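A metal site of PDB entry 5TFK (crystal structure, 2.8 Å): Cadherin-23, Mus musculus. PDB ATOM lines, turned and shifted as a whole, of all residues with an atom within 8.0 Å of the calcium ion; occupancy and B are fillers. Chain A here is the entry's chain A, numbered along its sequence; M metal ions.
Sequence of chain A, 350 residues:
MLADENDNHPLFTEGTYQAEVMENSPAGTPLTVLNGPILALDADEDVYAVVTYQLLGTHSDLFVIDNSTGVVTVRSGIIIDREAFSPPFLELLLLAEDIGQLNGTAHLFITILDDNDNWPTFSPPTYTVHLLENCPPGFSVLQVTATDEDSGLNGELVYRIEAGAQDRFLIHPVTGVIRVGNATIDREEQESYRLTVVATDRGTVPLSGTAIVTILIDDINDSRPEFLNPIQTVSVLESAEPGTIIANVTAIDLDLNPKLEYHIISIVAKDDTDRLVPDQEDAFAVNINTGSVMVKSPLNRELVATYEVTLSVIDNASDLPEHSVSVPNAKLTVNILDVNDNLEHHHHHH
OD1 of Asn 6 is bound to the calcium ion, 2.3 Å away. The calcium ion is bound by the side-chain carboxylate (OD2) of Asp 44, 2.4 Å away. The side-chain carboxylate (OD2) of Asp 98 binds the calcium ion. O of Tyr 48 is bound to the calcium ion (2.4 Å). The calcium ion is bound by O of Asn 8. The calcium ion is bound by OD2 of Asp 42, 2.5 Å away. The side-chain carboxylate (OD1) of Asp 42 binds the calcium ion, at 2.7 Å. The calcium ion has seven donor atoms within binding distance.
Six residues have an atom within 4 Å of the calcium ion: Asn 6, Asn 8, Asp 42, Asp 44, Tyr 48 and Asp 98.
OD1 of Asp 44 sits at hydrogen-bond distance from N of Asp 7 (3.0 Å). N of Leu 102 is in hydrogen-bond range of OD1 of Asp 98 (3.1 Å). OD1 of Asp 98 sits at hydrogen-bond distance from N of Gly 100 (2.8 Å). OD1 of Asp 98 sits at hydrogen-bond distance from N of Gln 101, at 3.1 Å.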
ATOM      1  N   GLU A   5       6.534  21.962  20.213  1.00  0.00           N
ATOM      2  CA  GLU A   5       5.079  21.657  20.422  1.00  0.00           C
ATOM      3  C   GLU A   5       4.524  20.313  19.854  1.00  0.00           C
ATOM      4  O   GLU A   5       3.392  19.917  20.196  1.00  0.00           O
ATOM      5  CB  GLU A   5       4.203  22.835  19.950  1.00  0.00           C
ATOM      6  CG  GLU A   5       4.103  23.992  20.947  1.00  0.00           C
ATOM      7  CD  GLU A   5       2.909  24.920  20.717  1.00  0.00           C
ATOM      8  OE1 GLU A   5       1.764  24.439  20.514  1.00  0.00           O
ATOM      9  OE2 GLU A   5       3.088  26.148  20.785  1.00  0.00           O
ATOM     10  N   ASN A   6       5.286  19.626  18.990  1.00  0.00           N
ATOM     11  CA  ASN A   6       4.956  18.275  18.473  1.00  0.00           C
ATOM     12  C   ASN A   6       5.826  17.173  19.158  1.00  0.00           C
ATOM     13  O   ASN A   6       6.563  16.439  18.499  1.00  0.00           O
ATOM     14  CB  ASN A   6       5.128  18.278  16.919  1.00  0.00           C
ATOM     15  CG  ASN A   6       4.437  17.097  16.211  1.00  0.00           C
ATOM     16  OD1 ASN A   6       3.570  16.415  16.759  1.00  0.00           O
ATOM     17  ND2 ASN A   6       4.816  16.859  14.953  1.00  0.00           N
ATOM     18  N   ASP A   7       5.721  17.053  20.487  1.00  0.00           N
ATOM     19  CA  ASP A   7       6.578  16.116  21.250  1.00  0.00           C
ATOM     20  C   ASP A   7       6.107  14.630  21.156  1.00  0.00           C
ATOM     21  O   ASP A   7       6.784  13.752  21.694  1.00  0.00           O
ATOM     22  CB  ASP A   7       6.719  16.548  22.733  1.00  0.00           C
ATOM     23  CG  ASP A   7       7.257  18.003  22.900  1.00  0.00           C
ATOM     24  OD1 ASP A   7       8.493  18.200  23.077  1.00  0.00           O
ATOM     25  OD2 ASP A   7       6.432  18.942  22.905  1.00  0.00           O
ATOM     26  N   ASN A   8       4.975  14.371  20.498  1.00  0.00           N
ATOM     27  CA  ASN A   8       4.449  12.999  20.307  1.00  0.00           C
ATOM     28  C   ASN A   8       4.019  12.676  18.871  1.00  0.00           C
ATOM     29  O   ASN A   8       3.758  13.558  18.043  1.00  0.00           O
ATOM     30  CB  ASN A   8       3.228  12.722  21.201  1.00  0.00           C
ATOM     31  CG  ASN A   8       3.494  12.998  22.654  1.00  0.00           C
ATOM     32  OD1 ASN A   8       3.682  12.085  23.438  1.00  0.00           O
ATOM     33  ND2 ASN A   8       3.520  14.268  23.018  1.00  0.00           N
ATOM     34  N   HIS A   9       3.882  11.380  18.626  1.00  0.00           N
ATOM     35  CA  HIS A   9       3.397  10.861  17.358  1.00  0.00           C
ATOM     36  C   HIS A   9       2.150   9.999  17.647  1.00  0.00           C
ATOM     37  O   HIS A   9       1.874   9.643  18.805  1.00  0.00           O
ATOM     38  CB  HIS A   9       4.517  10.067  16.645  1.00  0.00           C
ATOM     39  CG  HIS A   9       5.018   8.890  17.430  1.00  0.00           C
ATOM     40  ND1 HIS A   9       4.615   7.597  17.166  1.00  0.00           N
ATOM     41  CD2 HIS A   9       5.879   8.818  18.470  1.00  0.00           C
ATOM     42  CE1 HIS A   9       5.218   6.777  18.011  1.00  0.00           C
ATOM     43  NE2 HIS A   9       5.985   7.485  18.813  1.00  0.00           N
ATOM     44  N   PRO A  10       1.359   9.703  16.593  1.00  0.00           N
ATOM     45  CA  PRO A  10       0.160   8.915  16.812  1.00  0.00           C
ATOM     46  C   PRO A  10       0.464   7.470  17.213  1.00  0.00           C
ATOM     47  O   PRO A  10       1.572   6.970  16.991  1.00  0.00           O
ATOM     48  CB  PRO A  10      -0.558   8.950  15.448  1.00  0.00           C
ATOM     49  CG  PRO A  10       0.183   9.924  14.598  1.00  0.00           C
ATOM     50  CD  PRO A  10       1.558  10.026  15.172  1.00  0.00           C
ATOM     51  N   LEU A  41      -4.288   7.671  18.237  1.00  0.00           N
ATOM     52  CA  LEU A  41      -4.283   8.766  19.197  1.00  0.00           C
ATOM     53  C   LEU A  41      -2.875   9.325  19.390  1.00  0.00           C
ATOM     54  O   LEU A  41      -1.886   8.570  19.551  1.00  0.00           O
ATOM     55  CB  LEU A  41      -4.824   8.299  20.536  1.00  0.00           C
ATOM     56  CG  LEU A  41      -6.293   7.877  20.520  1.00  0.00           C
ATOM     57  CD1 LEU A  41      -6.632   6.988  21.707  1.00  0.00           C
ATOM     58  CD2 LEU A  41      -7.179   9.098  20.501  1.00  0.00           C
ATOM     59  N   ASP A  42      -2.823  10.652  19.344  1.00  0.00           N
ATOM     60  CA  ASP A  42      -1.606  11.454  19.441  1.00  0.00           C
ATOM     61  C   ASP A  42      -1.720  12.458  20.596  1.00  0.00           C
ATOM     62  O   ASP A  42      -2.645  13.245  20.592  1.00  0.00           O
ATOM     63  CB  ASP A  42      -1.434  12.209  18.128  1.00  0.00           C
ATOM     64  CG  ASP A  42      -0.099  12.946  17.990  1.00  0.00           C
ATOM     65  OD1 ASP A  42       0.318  13.707  18.883  1.00  0.00           O
ATOM     66  OD2 ASP A  42       0.482  12.841  16.903  1.00  0.00           O
ATOM     67  N   ALA A  43      -0.801  12.389  21.556  1.00  0.00           N
ATOM     68  CA  ALA A  43      -1.011  13.019  22.860  1.00  0.00           C
ATOM     69  C   ALA A  43      -0.584  14.493  22.925  1.00  0.00           C
ATOM     70  O   ALA A  43      -0.649  15.080  23.992  1.00  0.00           O
ATOM     71  CB  ALA A  43      -0.326  12.210  23.945  1.00  0.00           C
ATOM     72  N   ASP A  44      -0.175  15.086  21.799  1.00  0.00           N
ATOM     73  CA  ASP A  44      -0.043  16.542  21.706  1.00  0.00           C
ATOM     74  C   ASP A  44      -1.377  17.261  21.895  1.00  0.00           C
ATOM     75  O   ASP A  44      -2.446  16.637  21.905  1.00  0.00           O
ATOM     76  CB  ASP A  44       0.549  16.958  20.353  1.00  0.00           C
ATOM     77  CG  ASP A  44       1.993  16.513  20.171  1.00  0.00           C
ATOM     78  OD1 ASP A  44       2.818  16.691  21.096  1.00  0.00           O
ATOM     79  OD2 ASP A  44       2.309  15.997  19.075  1.00  0.00           O
ATOM     80  N   GLU A  45      -1.300  18.576  22.088  1.00  0.00           N
ATOM     81  CA  GLU A  45      -2.492  19.417  22.200  1.00  0.00           C
ATOM     82  C   GLU A  45      -2.756  20.000  20.821  1.00  0.00           C
ATOM     83  O   GLU A  45      -1.852  20.033  19.982  1.00  0.00           O
ATOM     84  CB  GLU A  45      -2.254  20.573  23.189  1.00  0.00           C
ATOM     85  CG  GLU A  45      -2.811  20.378  24.594  1.00  0.00           C
ATOM     86  CD  GLU A  45      -2.963  21.687  25.362  1.00  0.00           C
ATOM     87  OE1 GLU A  45      -3.935  22.441  25.099  1.00  0.00           O
ATOM     88  OE2 GLU A  45      -2.119  21.955  26.241  1.00  0.00           O
ATOM     89  N   ASP A  46      -3.982  20.494  20.617  1.00  0.00           N
ATOM     90  CA  ASP A  46      -4.279  21.415  19.515  1.00  0.00           C
ATOM     91  C   ASP A  46      -4.049  20.709  18.176  1.00  0.00           C
ATOM     92  O   ASP A  46      -4.458  19.571  18.011  1.00  0.00           O
ATOM     93  CB  ASP A  46      -3.441  22.722  19.626  1.00  0.00           C
ATOM     94  CG  ASP A  46      -4.025  23.750  20.607  1.00  0.00           C
ATOM     95  OD1 ASP A  46      -5.179  23.583  21.071  1.00  0.00           O
ATOM     96  OD2 ASP A  46      -3.333  24.773  20.872  1.00  0.00           O
ATOM     97  N   VAL A  47      -3.332  21.368  17.271  1.00  0.00           N
ATOM     98  CA  VAL A  47      -3.204  20.972  15.869  1.00  0.00           C
ATOM     99  C   VAL A  47      -2.281  19.772  15.647  1.00  0.00           C
ATOM    100  O   VAL A  47      -2.372  19.103  14.625  1.00  0.00           O
ATOM    101  CB  VAL A  47      -2.715  22.168  15.005  1.00  0.00           C
ATOM    102  CG1 VAL A  47      -1.243  22.478  15.246  1.00  0.00           C
ATOM    103  CG2 VAL A  47      -2.966  21.932  13.525  1.00  0.00           C
ATOM    104  N   TYR A  48      -1.393  19.511  16.597  1.00  0.00           N
ATOM    105  CA  TYR A  48      -0.374  18.462  16.415  1.00  0.00           C
ATOM    106  C   TYR A  48      -0.930  17.095  16.842  1.00  0.00           C
ATOM    107  O   TYR A  48      -0.191  16.102  16.848  1.00  0.00           O
ATOM    108  CB  TYR A  48       0.919  18.802  17.193  1.00  0.00           C
ATOM    109  CG  TYR A  48       1.499  20.186  16.881  1.00  0.00           C
ATOM    110  CD1 TYR A  48       2.366  20.378  15.800  1.00  0.00           C
ATOM    111  CD2 TYR A  48       1.163  21.295  17.657  1.00  0.00           C
ATOM    112  CE1 TYR A  48       2.878  21.636  15.499  1.00  0.00           C
ATOM    113  CE2 TYR A  48       1.670  22.557  17.370  1.00  0.00           C
ATOM    114  CZ  TYR A  48       2.516  22.729  16.286  1.00  0.00           C
ATOM    115  OH  TYR A  48       3.011  23.991  16.016  1.00  0.00           O
ATOM    116  N   ALA A  49      -2.219  17.076  17.193  1.00  0.00           N
ATOM    117  CA  ALA A  49      -2.889  15.893  17.732  1.00  0.00           C
ATOM    118  C   ALA A  49      -3.814  15.240  16.715  1.00  0.00           C
ATOM    119  O   ALA A  49      -4.357  14.163  16.975  1.00  0.00           O
ATOM    120  CB  ALA A  49      -3.695  16.281  18.965  1.00  0.00           C
ATOM    121  N   VAL A  50      -3.994  15.873  15.568  1.00  0.00           N
ATOM    122  CA  VAL A  50      -4.878  15.351  14.542  1.00  0.00           C
ATOM    123  C   VAL A  50      -4.111  14.432  13.621  1.00  0.00           C
ATOM    124  O   VAL A  50      -2.994  14.724  13.127  1.00  0.00           O
ATOM    125  CB  VAL A  50      -5.601  16.453  13.736  1.00  0.00           C
ATOM    126  CG1 VAL A  50      -6.291  17.400  14.687  1.00  0.00           C
ATOM    127  CG2 VAL A  50      -4.653  17.210  12.826  1.00  0.00           C
ATOM    128  N   VAL A  51      -4.780  13.319  13.318  1.00  0.00           N
ATOM    129  CA  VAL A  51      -4.217  12.229  12.484  1.00  0.00           C
ATOM    130  C   VAL A  51      -4.926  12.037  11.141  1.00  0.00           C
ATOM    131  O   VAL A  51      -6.126  12.273  10.979  1.00  0.00           O
ATOM    132  CB  VAL A  51      -4.245  10.865  13.195  1.00  0.00           C
ATOM    133  CG1 VAL A  51      -3.314  10.882  14.381  1.00  0.00           C
ATOM    134  CG2 VAL A  51      -5.643  10.470  13.659  1.00  0.00           C
ATOM    135  N   GLU A  97      -0.353   9.555  10.483  1.00  0.00           N
ATOM    136  CA  GLU A  97       0.523  10.713  10.311  1.00  0.00           C
ATOM    137  C   GLU A  97      -0.094  11.930  11.021  1.00  0.00           C
ATOM    138  O   GLU A  97      -1.280  12.256  10.843  1.00  0.00           O
ATOM    139  CB  GLU A  97       0.717  11.071   8.832  1.00  0.00           C
ATOM    140  CG  GLU A  97       1.388  10.019   7.954  1.00  0.00           C
ATOM    141  CD  GLU A  97       2.523  10.594   7.100  1.00  0.00           C
ATOM    142  OE1 GLU A  97       2.433  10.587   5.843  1.00  0.00           O
ATOM    143  OE2 GLU A  97       3.539  11.058   7.685  1.00  0.00           O
ATOM    144  N   ASP A  98       0.694  12.590  11.858  1.00  0.00           N
ATOM    145  CA  ASP A  98       0.425  14.003  12.211  1.00  0.00           C
ATOM    146  C   ASP A  98       0.937  15.045  11.201  1.00  0.00           C
ATOM    147  O   ASP A  98       1.638  14.739  10.210  1.00  0.00           O
ATOM    148  CB  ASP A  98       0.869  14.323  13.646  1.00  0.00           C
ATOM    149  CG  ASP A  98       2.390  14.493  13.800  1.00  0.00           C
ATOM    150  OD1 ASP A  98       3.107  14.873  12.840  1.00  0.00           O
ATOM    151  OD2 ASP A  98       2.851  14.308  14.945  1.00  0.00           O
ATOM    152  N   ILE A  99       0.563  16.309  11.433  1.00  0.00           N
ATOM    153  CA  ILE A  99       0.882  17.378  10.481  1.00  0.00           C
ATOM    154  C   ILE A  99       2.397  17.665  10.324  1.00  0.00           C
ATOM    155  O   ILE A  99       2.820  18.185   9.299  1.00  0.00           O
ATOM    156  CB  ILE A  99       0.047  18.665  10.746  1.00  0.00           C
ATOM    157  CG1 ILE A  99      -0.020  19.574   9.504  1.00  0.00           C
ATOM    158  CG2 ILE A  99       0.576  19.434  11.953  1.00  0.00           C
ATOM    159  CD1 ILE A  99      -0.616  18.934   8.246  1.00  0.00           C
ATOM    160  N   GLY A 100       3.208  17.265  11.301  1.00  0.00           N
ATOM    161  CA  GLY A 100       4.672  17.295  11.156  1.00  0.00           C
ATOM    162  C   GLY A 100       5.288  16.098  10.456  1.00  0.00           C
ATOM    163  O   GLY A 100       6.505  16.038  10.300  1.00  0.00           O
ATOM    164  N   GLN A 101       4.443  15.158  10.017  1.00  0.00           N
ATOM    165  CA  GLN A 101       4.840  13.895   9.357  1.00  0.00           C
ATOM    166  C   GLN A 101       5.450  12.856  10.314  1.00  0.00           C
ATOM    167  O   GLN A 101       6.274  12.050   9.870  1.00  0.00           O
ATOM    168  CB  GLN A 101       5.746  14.132   8.124  1.00  0.00           C
ATOM    169  CG  GLN A 101       5.138  15.017   7.027  1.00  0.00           C
ATOM    170  CD  GLN A 101       4.152  14.286   6.115  1.00  0.00           C
ATOM    171  OE1 GLN A 101       4.504  13.846   5.022  1.00  0.00           O
ATOM    172  NE2 GLN A 101       2.897  14.154   6.569  1.00  0.00           N
ATOM    173  N   LEU A 102       5.027  12.841  11.579  1.00  0.00           N
ATOM    174  CA  LEU A 102       5.361  11.792  12.532  1.00  0.00           C
ATOM    175  C   LEU A 102       4.316  10.684  12.524  1.00  0.00           C
ATOM    176  O   LEU A 102       3.097  10.912  12.474  1.00  0.00           O
ATOM    177  CB  LEU A 102       5.528  12.351  13.946  1.00  0.00           C
ATOM    178  CG  LEU A 102       6.463  13.558  14.112  1.00  0.00           C
ATOM    179  CD1 LEU A 102       6.577  13.917  15.586  1.00  0.00           C
ATOM    180  CD2 LEU A 102       7.847  13.339  13.538  1.00  0.00           C
ATOM    181  N   ASN A 103       4.803   9.457  12.677  1.00  0.00           N
ATOM    182  CA  ASN A 103       4.093   8.226  12.286  1.00  0.00           C
ATOM    183  C   ASN A 103       3.686   7.303  13.417  1.00  0.00           C
ATOM    184  O   ASN A 103       4.346   7.189  14.412  1.00  0.00           O
ATOM    185  CB  ASN A 103       4.988   7.349  11.420  1.00  0.00           C
ATOM    186  CG  ASN A 103       5.215   7.941  10.068  1.00  0.00           C
ATOM    187  OD1 ASN A 103       6.364   8.223   9.682  1.00  0.00           O
ATOM    188  ND2 ASN A 103       4.127   8.208   9.350  1.00  0.00           N
HETATM  189 CA    CA M   1       1.907  14.878  17.037  1.00  0.00          CA
